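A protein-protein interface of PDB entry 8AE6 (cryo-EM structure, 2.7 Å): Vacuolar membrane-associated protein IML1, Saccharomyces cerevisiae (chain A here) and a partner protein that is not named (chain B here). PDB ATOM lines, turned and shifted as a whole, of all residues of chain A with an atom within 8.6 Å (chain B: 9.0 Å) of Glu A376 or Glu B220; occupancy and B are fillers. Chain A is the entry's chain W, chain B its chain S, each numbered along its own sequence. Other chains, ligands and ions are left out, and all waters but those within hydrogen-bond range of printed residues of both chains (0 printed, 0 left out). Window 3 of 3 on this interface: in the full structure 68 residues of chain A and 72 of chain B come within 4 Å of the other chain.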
ATOM      1  N   VAL A 304     -16.742  -9.070  32.158  1.00  0.00           N
ATOM      2  CA  VAL A 304     -15.339  -9.461  32.054  1.00  0.00           C
ATOM      3  C   VAL A 304     -14.497  -9.041  33.251  1.00  0.00           C
ATOM      4  O   VAL A 304     -13.331  -9.459  33.342  1.00  0.00           O
ATOM      5  CB  VAL A 304     -14.689  -8.913  30.766  1.00  0.00           C
ATOM      6  CG1 VAL A 304     -15.538  -9.238  29.560  1.00  0.00           C
ATOM      7  CG2 VAL A 304     -14.448  -7.416  30.880  1.00  0.00           C
ATOM      8  N   PHE A 328     -20.003 -16.336  21.679  1.00  0.00           N
ATOM      9  CA  PHE A 328     -20.830 -15.155  21.507  1.00  0.00           C
ATOM     10  C   PHE A 328     -22.114 -15.518  20.769  1.00  0.00           C
ATOM     11  O   PHE A 328     -22.244 -16.591  20.174  1.00  0.00           O
ATOM     12  CB  PHE A 328     -20.079 -14.067  20.739  1.00  0.00           C
ATOM     13  CG  PHE A 328     -18.938 -13.457  21.500  1.00  0.00           C
ATOM     14  CD1 PHE A 328     -18.897 -13.504  22.878  1.00  0.00           C
ATOM     15  CD2 PHE A 328     -17.913 -12.815  20.827  1.00  0.00           C
ATOM     16  CE1 PHE A 328     -17.851 -12.936  23.573  1.00  0.00           C
ATOM     17  CE2 PHE A 328     -16.866 -12.241  21.514  1.00  0.00           C
ATOM     18  CZ  PHE A 328     -16.835 -12.304  22.890  1.00  0.00           C
ATOM     19  N   ARG A 356     -20.252 -16.497  17.365  1.00  0.00           N
ATOM     20  CA  ARG A 356     -18.793 -16.486  17.427  1.00  0.00           C
ATOM     21  C   ARG A 356     -18.366 -17.313  18.633  1.00  0.00           C
ATOM     22  O   ARG A 356     -18.539 -16.886  19.780  1.00  0.00           O
ATOM     23  CB  ARG A 356     -18.267 -15.053  17.516  1.00  0.00           C
ATOM     24  CG  ARG A 356     -16.792 -14.913  17.865  1.00  0.00           C
ATOM     25  CD  ARG A 356     -15.896 -15.539  16.817  1.00  0.00           C
ATOM     26  NE  ARG A 356     -14.486 -15.285  17.073  1.00  0.00           N
ATOM     27  CZ  ARG A 356     -13.493 -15.986  16.544  1.00  0.00           C
ATOM     28  NH1 ARG A 356     -13.723 -17.003  15.733  1.00  0.00           N
ATOM     29  NH2 ARG A 356     -12.237 -15.659  16.834  1.00  0.00           N
ATOM     30  N   VAL A 358     -15.808 -18.305  21.022  1.00  0.00           N
ATOM     31  CA  VAL A 358     -14.535 -17.739  21.458  1.00  0.00           C
ATOM     32  C   VAL A 358     -13.612 -18.828  21.978  1.00  0.00           C
ATOM     33  O   VAL A 358     -12.525 -19.059  21.438  1.00  0.00           O
ATOM     34  CB  VAL A 358     -14.771 -16.658  22.523  1.00  0.00           C
ATOM     35  CG1 VAL A 358     -13.466 -16.022  22.895  1.00  0.00           C
ATOM     36  CG2 VAL A 358     -15.743 -15.627  22.012  1.00  0.00           C
ATOM     37  N   ASP A 369      -5.597 -17.909  29.597  1.00  0.00           N
ATOM     38  CA  ASP A 369      -5.780 -17.950  28.149  1.00  0.00           C
ATOM     39  C   ASP A 369      -7.245 -17.769  27.770  1.00  0.00           C
ATOM     40  O   ASP A 369      -7.555 -17.122  26.760  1.00  0.00           O
ATOM     41  CB  ASP A 369      -5.239 -19.268  27.595  1.00  0.00           C
ATOM     42  CG  ASP A 369      -5.585 -19.472  26.135  1.00  0.00           C
ATOM     43  OD1 ASP A 369      -4.886 -18.904  25.270  1.00  0.00           O
ATOM     44  OD2 ASP A 369      -6.558 -20.203  25.850  1.00  0.00           O
ATOM     45  N   ILE A 370      -8.151 -18.322  28.580  1.00  0.00           N
ATOM     46  CA  ILE A 370      -9.587 -18.187  28.332  1.00  0.00           C
ATOM     47  C   ILE A 370     -10.008 -16.724  28.410  1.00  0.00           C
ATOM     48  O   ILE A 370     -10.699 -16.208  27.522  1.00  0.00           O
ATOM     49  CB  ILE A 370     -10.380 -19.057  29.322  1.00  0.00           C
ATOM     50  CG1 ILE A 370     -10.239 -20.538  28.971  1.00  0.00           C
ATOM     51  CG2 ILE A 370     -11.842 -18.662  29.349  1.00  0.00           C
ATOM     52  CD1 ILE A 370     -10.424 -21.457  30.147  1.00  0.00           C
ATOM     53  N   MET A 371      -9.563 -16.023  29.457  1.00  0.00           N
ATOM     54  CA  MET A 371      -9.896 -14.614  29.616  1.00  0.00           C
ATOM     55  C   MET A 371      -9.243 -13.759  28.537  1.00  0.00           C
ATOM     56  O   MET A 371      -9.855 -12.796  28.053  1.00  0.00           O
ATOM     57  CB  MET A 371      -9.483 -14.127  31.005  1.00  0.00           C
ATOM     58  CG  MET A 371     -10.391 -14.592  32.133  1.00  0.00           C
ATOM     59  SD  MET A 371     -12.139 -14.547  31.715  1.00  0.00           S
ATOM     60  CE  MET A 371     -12.435 -12.783  31.687  1.00  0.00           C
ATOM     61  N   GLU A 372      -8.008 -14.094  28.146  1.00  0.00           N
ATOM     62  CA  GLU A 372      -7.327 -13.346  27.092  1.00  0.00           C
ATOM     63  C   GLU A 372      -8.066 -13.457  25.764  1.00  0.00           C
ATOM     64  O   GLU A 372      -8.306 -12.449  25.083  1.00  0.00           O
ATOM     65  CB  GLU A 372      -5.889 -13.843  26.953  1.00  0.00           C
ATOM     66  CG  GLU A 372      -4.868 -13.030  27.725  1.00  0.00           C
ATOM     67  CD  GLU A 372      -3.495 -13.673  27.726  1.00  0.00           C
ATOM     68  OE1 GLU A 372      -3.372 -14.818  27.245  1.00  0.00           O
ATOM     69  OE2 GLU A 372      -2.539 -13.030  28.210  1.00  0.00           O
ATOM     70  N   THR A 373      -8.457 -14.683  25.395  1.00  0.00           N
ATOM     71  CA  THR A 373      -9.207 -14.891  24.162  1.00  0.00           C
ATOM     72  C   THR A 373     -10.572 -14.220  24.221  1.00  0.00           C
ATOM     73  O   THR A 373     -11.017 -13.632  23.228  1.00  0.00           O
ATOM     74  CB  THR A 373      -9.361 -16.385  23.887  1.00  0.00           C
ATOM     75  OG1 THR A 373      -8.116 -17.046  24.134  1.00  0.00           O
ATOM     76  CG2 THR A 373      -9.765 -16.621  22.445  1.00  0.00           C
ATOM     77  N   LEU A 374     -11.242 -14.281  25.381  1.00  0.00           N
ATOM     78  CA  LEU A 374     -12.555 -13.661  25.523  1.00  0.00           C
ATOM     79  C   LEU A 374     -12.479 -12.152  25.352  1.00  0.00           C
ATOM     80  O   LEU A 374     -13.288 -11.561  24.623  1.00  0.00           O
ATOM     81  CB  LEU A 374     -13.156 -14.026  26.882  1.00  0.00           C
ATOM     82  CG  LEU A 374     -14.643 -13.779  27.157  1.00  0.00           C
ATOM     83  CD1 LEU A 374     -15.162 -14.844  28.083  1.00  0.00           C
ATOM     84  CD2 LEU A 374     -14.899 -12.417  27.777  1.00  0.00           C
ATOM     85  N   ARG A 375     -11.491 -11.515  25.984  1.00  0.00           N
ATOM     86  CA  ARG A 375     -11.361 -10.068  25.887  1.00  0.00           C
ATOM     87  C   ARG A 375     -10.971  -9.631  24.478  1.00  0.00           C
ATOM     88  O   ARG A 375     -11.521  -8.650  23.956  1.00  0.00           O
ATOM     89  CB  ARG A 375     -10.357  -9.577  26.925  1.00  0.00           C
ATOM     90  CG  ARG A 375     -10.884  -9.683  28.347  1.00  0.00           C
ATOM     91  CD  ARG A 375      -9.787  -9.585  29.389  1.00  0.00           C
ATOM     92  NE  ARG A 375     -10.206  -8.746  30.504  1.00  0.00           N
ATOM     93  CZ  ARG A 375     -10.323  -9.162  31.755  1.00  0.00           C
ATOM     94  NH1 ARG A 375     -10.041 -10.406  32.099  1.00  0.00           N
ATOM     95  NH2 ARG A 375     -10.728  -8.309  32.689  1.00  0.00           N
ATOM     96  N   GLU A 376     -10.054 -10.366  23.833  1.00  0.00           N
ATOM     97  CA  GLU A 376      -9.658 -10.022  22.468  1.00  0.00           C
ATOM     98  C   GLU A 376     -10.816 -10.175  21.488  1.00  0.00           C
ATOM     99  O   GLU A 376     -11.041  -9.299  20.638  1.00  0.00           O
ATOM    100  CB  GLU A 376      -8.478 -10.889  22.031  1.00  0.00           C
ATOM    101  CG  GLU A 376      -7.120 -10.261  22.277  1.00  0.00           C
ATOM    102  CD  GLU A 376      -5.979 -11.146  21.819  1.00  0.00           C
ATOM    103  OE1 GLU A 376      -6.247 -12.149  21.125  1.00  0.00           O
ATOM    104  OE2 GLU A 376      -4.815 -10.839  22.152  1.00  0.00           O
ATOM    105  N   GLU A 377     -11.581 -11.263  21.604  1.00  0.00           N
ATOM    106  CA  GLU A 377     -12.682 -11.473  20.675  1.00  0.00           C
ATOM    107  C   GLU A 377     -13.832 -10.508  20.930  1.00  0.00           C
ATOM    108  O   GLU A 377     -14.504 -10.091  19.976  1.00  0.00           O
ATOM    109  CB  GLU A 377     -13.158 -12.920  20.744  1.00  0.00           C
ATOM    110  CG  GLU A 377     -12.153 -13.904  20.172  1.00  0.00           C
ATOM    111  CD  GLU A 377     -11.477 -13.386  18.916  1.00  0.00           C
ATOM    112  OE1 GLU A 377     -12.173 -13.207  17.894  1.00  0.00           O
ATOM    113  OE2 GLU A 377     -10.250 -13.158  18.953  1.00  0.00           O
ATOM    114  N   PHE A 378     -14.062 -10.117  22.186  1.00  0.00           N
ATOM    115  CA  PHE A 378     -15.079  -9.108  22.435  1.00  0.00           C
ATOM    116  C   PHE A 378     -14.655  -7.746  21.914  1.00  0.00           C
ATOM    117  O   PHE A 378     -15.507  -6.965  21.474  1.00  0.00           O
ATOM    118  CB  PHE A 378     -15.419  -9.022  23.922  1.00  0.00           C
ATOM    119  CG  PHE A 378     -16.773  -8.437  24.185  1.00  0.00           C
ATOM    120  CD1 PHE A 378     -17.887  -9.253  24.258  1.00  0.00           C
ATOM    121  CD2 PHE A 378     -16.941  -7.070  24.318  1.00  0.00           C
ATOM    122  CE1 PHE A 378     -19.138  -8.719  24.482  1.00  0.00           C
ATOM    123  CE2 PHE A 378     -18.188  -6.531  24.531  1.00  0.00           C
ATOM    124  CZ  PHE A 378     -19.287  -7.357  24.620  1.00  0.00           C
ATOM    125  N   MET A 379     -13.358  -7.435  21.947  1.00  0.00           N
ATOM    126  CA  MET A 379     -12.917  -6.180  21.349  1.00  0.00           C
ATOM    127  C   MET A 379     -12.973  -6.227  19.826  1.00  0.00           C
ATOM    128  O   MET A 379     -13.135  -5.184  19.182  1.00  0.00           O
ATOM    129  CB  MET A 379     -11.509  -5.833  21.819  1.00  0.00           C
ATOM    130  CG  MET A 379     -11.449  -5.285  23.229  1.00  0.00           C
ATOM    131  SD  MET A 379     -12.273  -3.697  23.412  1.00  0.00           S
ATOM    132  CE  MET A 379     -12.824  -3.805  25.111  1.00  0.00           C
ATOM    133  N   GLU A 380     -12.842  -7.413  19.229  1.00  0.00           N
ATOM    134  CA  GLU A 380     -12.845  -7.525  17.775  1.00  0.00           C
ATOM    135  C   GLU A 380     -14.226  -7.756  17.162  1.00  0.00           C
ATOM    136  O   GLU A 380     -14.357  -7.656  15.934  1.00  0.00           O
ATOM    137  CB  GLU A 380     -11.916  -8.659  17.338  1.00  0.00           C
ATOM    138  CG  GLU A 380     -10.442  -8.313  17.395  1.00  0.00           C
ATOM    139  CD  GLU A 380      -9.564  -9.407  16.823  1.00  0.00           C
ATOM    140  OE1 GLU A 380     -10.114 -10.392  16.286  1.00  0.00           O
ATOM    141  OE2 GLU A 380      -8.324  -9.283  16.905  1.00  0.00           O
ATOM    142  N   ILE A 381     -15.244  -8.066  17.972  1.00  0.00           N
ATOM    143  CA  ILE A 381     -16.551  -8.432  17.420  1.00  0.00           C
ATOM    144  C   ILE A 381     -17.238  -7.253  16.719  1.00  0.00           C
ATOM    145  O   ILE A 381     -17.981  -7.455  15.745  1.00  0.00           O
ATOM    146  CB  ILE A 381     -17.425  -9.064  18.528  1.00  0.00           C
ATOM    147  CG1 ILE A 381     -18.521  -9.936  17.924  1.00  0.00           C
ATOM    148  CG2 ILE A 381     -18.018  -8.028  19.475  1.00  0.00           C
ATOM    149  CD1 ILE A 381     -18.006 -11.185  17.249  1.00  0.00           C
ATOM    150  N   ARG A 382     -16.973  -6.015  17.152  1.00  0.00           N
ATOM    151  CA  ARG A 382     -17.592  -4.854  16.517  1.00  0.00           C
ATOM    152  C   ARG A 382     -17.060  -4.640  15.107  1.00  0.00           C
ATOM    153  O   ARG A 382     -17.835  -4.380  14.179  1.00  0.00           O
ATOM    154  CB  ARG A 382     -17.361  -3.600  17.356  1.00  0.00           C
ATOM    155  CG  ARG A 382     -17.990  -3.636  18.725  1.00  0.00           C
ATOM    156  CD  ARG A 382     -18.334  -2.237  19.193  1.00  0.00           C
ATOM    157  NE  ARG A 382     -19.711  -1.886  18.866  1.00  0.00           N
ATOM    158  CZ  ARG A 382     -20.211  -0.661  18.946  1.00  0.00           C
ATOM    159  NH1 ARG A 382     -19.474   0.364  19.342  1.00  0.00           N
ATOM    160  NH2 ARG A 382     -21.485  -0.459  18.621  1.00  0.00           N
ATOM    161  N   ASP A 384     -15.748  -7.049  13.382  1.00  0.00           N
ATOM    162  CA  ASP A 384     -16.148  -8.239  12.638  1.00  0.00           C
ATOM    163  C   ASP A 384     -17.552  -8.100  12.063  1.00  0.00           C
ATOM    164  O   ASP A 384     -17.809  -8.534  10.934  1.00  0.00           O
ATOM    165  CB  ASP A 384     -16.061  -9.472  13.535  1.00  0.00           C
ATOM    166  CG  ASP A 384     -14.636  -9.951  13.724  1.00  0.00           C
ATOM    167  OD1 ASP A 384     -13.752  -9.510  12.961  1.00  0.00           O
ATOM    168  OD2 ASP A 384     -14.401 -10.771  14.639  1.00  0.00           O
ATOM    169  N   GLN B 121      -4.362 -11.855  36.464  1.00  0.00           N
ATOM    170  CA  GLN B 121      -4.459 -12.703  35.280  1.00  0.00           C
ATOM    171  C   GLN B 121      -3.131 -12.822  34.540  1.00  0.00           C
ATOM    172  O   GLN B 121      -2.588 -13.924  34.410  1.00  0.00           O
ATOM    173  CB  GLN B 121      -5.543 -12.157  34.345  1.00  0.00           C
ATOM    174  CG  GLN B 121      -5.826 -13.033  33.145  1.00  0.00           C
ATOM    175  CD  GLN B 121      -6.336 -12.243  31.963  1.00  0.00           C
ATOM    176  OE1 GLN B 121      -6.758 -11.098  32.103  1.00  0.00           O
ATOM    177  NE2 GLN B 121      -6.305 -12.853  30.785  1.00  0.00           N
ATOM    178  N   ASN B 122      -2.589 -11.705  34.057  1.00  0.00           N
ATOM    179  CA  ASN B 122      -1.420 -11.749  33.185  1.00  0.00           C
ATOM    180  C   ASN B 122      -0.225 -10.982  33.733  1.00  0.00           C
ATOM    181  O   ASN B 122       0.779 -10.849  33.018  1.00  0.00           O
ATOM    182  CB  ASN B 122      -1.777 -11.231  31.788  1.00  0.00           C
ATOM    183  CG  ASN B 122      -2.018  -9.736  31.758  1.00  0.00           C
ATOM    184  OD1 ASN B 122      -1.095  -8.952  31.535  1.00  0.00           O
ATOM    185  ND2 ASN B 122      -3.263  -9.335  31.968  1.00  0.00           N
ATOM    186  N   LEU B 124       0.266  -7.640  34.615  1.00  0.00           N
ATOM    187  CA  LEU B 124       0.481  -6.498  33.738  1.00  0.00           C
ATOM    188  C   LEU B 124       1.350  -5.431  34.400  1.00  0.00           C
ATOM    189  O   LEU B 124       2.420  -5.080  33.886  1.00  0.00           O
ATOM    190  CB  LEU B 124      -0.888  -5.947  33.316  1.00  0.00           C
ATOM    191  CG  LEU B 124      -1.098  -4.828  32.305  1.00  0.00           C
ATOM    192  CD1 LEU B 124      -2.412  -5.043  31.611  1.00  0.00           C
ATOM    193  CD2 LEU B 124      -1.170  -3.521  33.044  1.00  0.00           C
ATOM    194  N   PHE B 195       2.972  -1.493  26.450  1.00  0.00           N
ATOM    195  CA  PHE B 195       2.057  -0.721  27.281  1.00  0.00           C
ATOM    196  C   PHE B 195       2.828   0.253  28.166  1.00  0.00           C
ATOM    197  O   PHE B 195       3.835  -0.109  28.772  1.00  0.00           O
ATOM    198  CB  PHE B 195       1.198  -1.653  28.139  1.00  0.00           C
ATOM    199  CG  PHE B 195       0.403  -0.939  29.186  1.00  0.00           C
ATOM    200  CD1 PHE B 195      -0.511   0.042  28.831  1.00  0.00           C
ATOM    201  CD2 PHE B 195       0.579  -1.229  30.524  1.00  0.00           C
ATOM    202  CE1 PHE B 195      -1.234   0.709  29.796  1.00  0.00           C
ATOM    203  CE2 PHE B 195      -0.141  -0.560  31.489  1.00  0.00           C
ATOM    204  CZ  PHE B 195      -1.049   0.403  31.124  1.00  0.00           C
ATOM    205  N   PRO B 217      -7.320   2.106  24.885  1.00  0.00           N
ATOM    206  CA  PRO B 217      -6.898   0.704  24.786  1.00  0.00           C
ATOM    207  C   PRO B 217      -5.506   0.511  25.367  1.00  0.00           C
ATOM    208  O   PRO B 217      -4.568   1.237  25.029  1.00  0.00           O
ATOM    209  CB  PRO B 217      -6.922   0.427  23.278  1.00  0.00           C
ATOM    210  CG  PRO B 217      -7.630   1.589  22.667  1.00  0.00           C
ATOM    211  CD  PRO B 217      -7.400   2.746  23.565  1.00  0.00           C
ATOM    212  N   ILE B 218      -5.381  -0.477  26.246  1.00  0.00           N
ATOM    213  CA  ILE B 218      -4.102  -0.797  26.861  1.00  0.00           C
ATOM    214  C   ILE B 218      -3.541  -2.126  26.380  1.00  0.00           C
ATOM    215  O   ILE B 218      -2.352  -2.395  26.610  1.00  0.00           O
ATOM    216  CB  ILE B 218      -4.205  -0.788  28.400  1.00  0.00           C
ATOM    217  CG1 ILE B 218      -5.086  -1.936  28.886  1.00  0.00           C
ATOM    218  CG2 ILE B 218      -4.761   0.537  28.881  1.00  0.00           C
ATOM    219  CD1 ILE B 218      -5.276  -1.963  30.379  1.00  0.00           C
ATOM    220  N   ASP B 219      -4.339  -2.956  25.717  1.00  0.00           N
ATOM    221  CA  ASP B 219      -3.895  -4.244  25.212  1.00  0.00           C
ATOM    222  C   ASP B 219      -4.688  -4.557  23.950  1.00  0.00           C
ATOM    223  O   ASP B 219      -5.346  -3.685  23.378  1.00  0.00           O
ATOM    224  CB  ASP B 219      -4.066  -5.341  26.271  1.00  0.00           C
ATOM    225  CG  ASP B 219      -2.876  -5.454  27.197  1.00  0.00           C
ATOM    226  OD1 ASP B 219      -1.735  -5.255  26.728  1.00  0.00           O
ATOM    227  OD2 ASP B 219      -3.079  -5.754  28.390  1.00  0.00           O
ATOM    228  N   GLU B 220      -4.622  -5.813  23.516  1.00  0.00           N
ATOM    229  CA  GLU B 220      -5.416  -6.268  22.384  1.00  0.00           C
ATOM    230  C   GLU B 220      -6.832  -6.657  22.779  1.00  0.00           C
ATOM    231  O   GLU B 220      -7.656  -6.903  21.893  1.00  0.00           O
ATOM    232  CB  GLU B 220      -4.729  -7.455  21.706  1.00  0.00           C
ATOM    233  CG  GLU B 220      -3.317  -7.164  21.227  1.00  0.00           C
ATOM    234  CD  GLU B 220      -2.258  -7.654  22.196  1.00  0.00           C
ATOM    235  OE1 GLU B 220      -2.593  -8.476  23.077  1.00  0.00           O
ATOM    236  OE2 GLU B 220      -1.096  -7.218  22.079  1.00  0.00           O
ATOM    237  N   GLY B 221      -7.132  -6.723  24.072  1.00  0.00           N
ATOM    238  CA  GLY B 221      -8.467  -7.053  24.520  1.00  0.00           C
ATOM    239  C   GLY B 221      -8.933  -6.234  25.706  1.00  0.00           C
ATOM    240  O   GLY B 221     -10.062  -6.400  26.174  1.00  0.00           O
ATOM    241  N   ASN B 222      -8.083  -5.338  26.192  1.00  0.00           N
ATOM    242  CA  ASN B 222      -8.373  -4.551  27.381  1.00  0.00           C
ATOM    243  C   ASN B 222      -8.346  -3.069  27.048  1.00  0.00           C
ATOM    244  O   ASN B 222      -7.481  -2.604  26.301  1.00  0.00           O
ATOM    245  CB  ASN B 222      -7.374  -4.850  28.493  1.00  0.00           C
ATOM    246  CG  ASN B 222      -7.587  -6.205  29.117  1.00  0.00           C
ATOM    247  OD1 ASN B 222      -8.617  -6.458  29.737  1.00  0.00           O
ATOM    248  ND2 ASN B 222      -6.611  -7.089  28.958  1.00  0.00           N
ATOM    249  N   ALA B 223      -9.299  -2.332  27.610  1.00  0.00           N
ATOM    250  CA  ALA B 223      -9.369  -0.894  27.433  1.00  0.00           C
ATOM    251  C   ALA B 223      -9.975  -0.276  28.679  1.00  0.00           C
ATOM    252  O   ALA B 223     -10.737  -0.924  29.402  1.00  0.00           O
ATOM    253  CB  ALA B 223     -10.195  -0.515  26.198  1.00  0.00           C
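The backbone carbonyl oxygen of Val A304 lies within hydrogen-bond range of the guanidinium group of Arg A375 (2.9 Å).
Of the printed residues of chain B, Met A371 touches Gln B121 (3.4 Å). Printed residues of chain B within 4 Å of Glu A372: Gln B121 (3.4 Å). Of chain B, only Glu B220 (3.4 Å) and Gly B221 (3.7 Å) come within 4 Å of Glu A376. Glu A377 touches none of the printed residues of chain B. Ile A381 touches none of the printed residues of chain B. Pro B217 touches none of the printed residues of chain A. Printed residues of chain A within 4 Å of Glu B220: Glu A376 and Met A379. The nearest residue of chain B that does not touch Glu A376 is Asn B222 (5.9 Å). The nearest printed residue of chain A that does not touch Glu B220 is Arg A375 (4.7 Å). The nearest printed residue of chain B that does not touch Met A371 is Asn B222 (6.6 Å).
Printed residues of chain B that touch a printed residue of chain A: Gln B121, Glu B220, Gly B221 and Asn B222. Of the 19 printed residues of chain A, 5 touch a printed residue of chain B. Printed residues of chain A that touch a printed residue of chain B: Met A371, Glu A372, Arg A375, Glu A376 and Met A379. Hydrophobic or aromatic side chains of chain A that line the printed part of chain B: Met A371 and Met A379. Among the printed residues, 9 pairs touch across the chains.
Among the printed residues, pairs that only touch across the chains: Met A371 with Gln B121 (3.4 Å), Met A379 with Gly B221 (3.4 Å), Glu A376 with Gly B221 (3.7 Å) and Met A379 with Glu B220 (3.999 Å).
The backbone NH of Glu A372 lies close to the side-chain amide nitrogen of Gln B121 (3.4 Å). The side-chain amide oxygen of Gln B121 sits at hydrogen-bond distance from the guanidinium group of Arg A375, 3.4 Å away. The guanidinium group of Arg A375 lies within hydrogen-bond range of the side-chain amide oxygen of Asn B222, at 2.9 Å. O of Arg A375 lies close to O of Gly B221. OE2 of Glu A376 lies close to OE1 of Glu B220 (3.4 Å).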
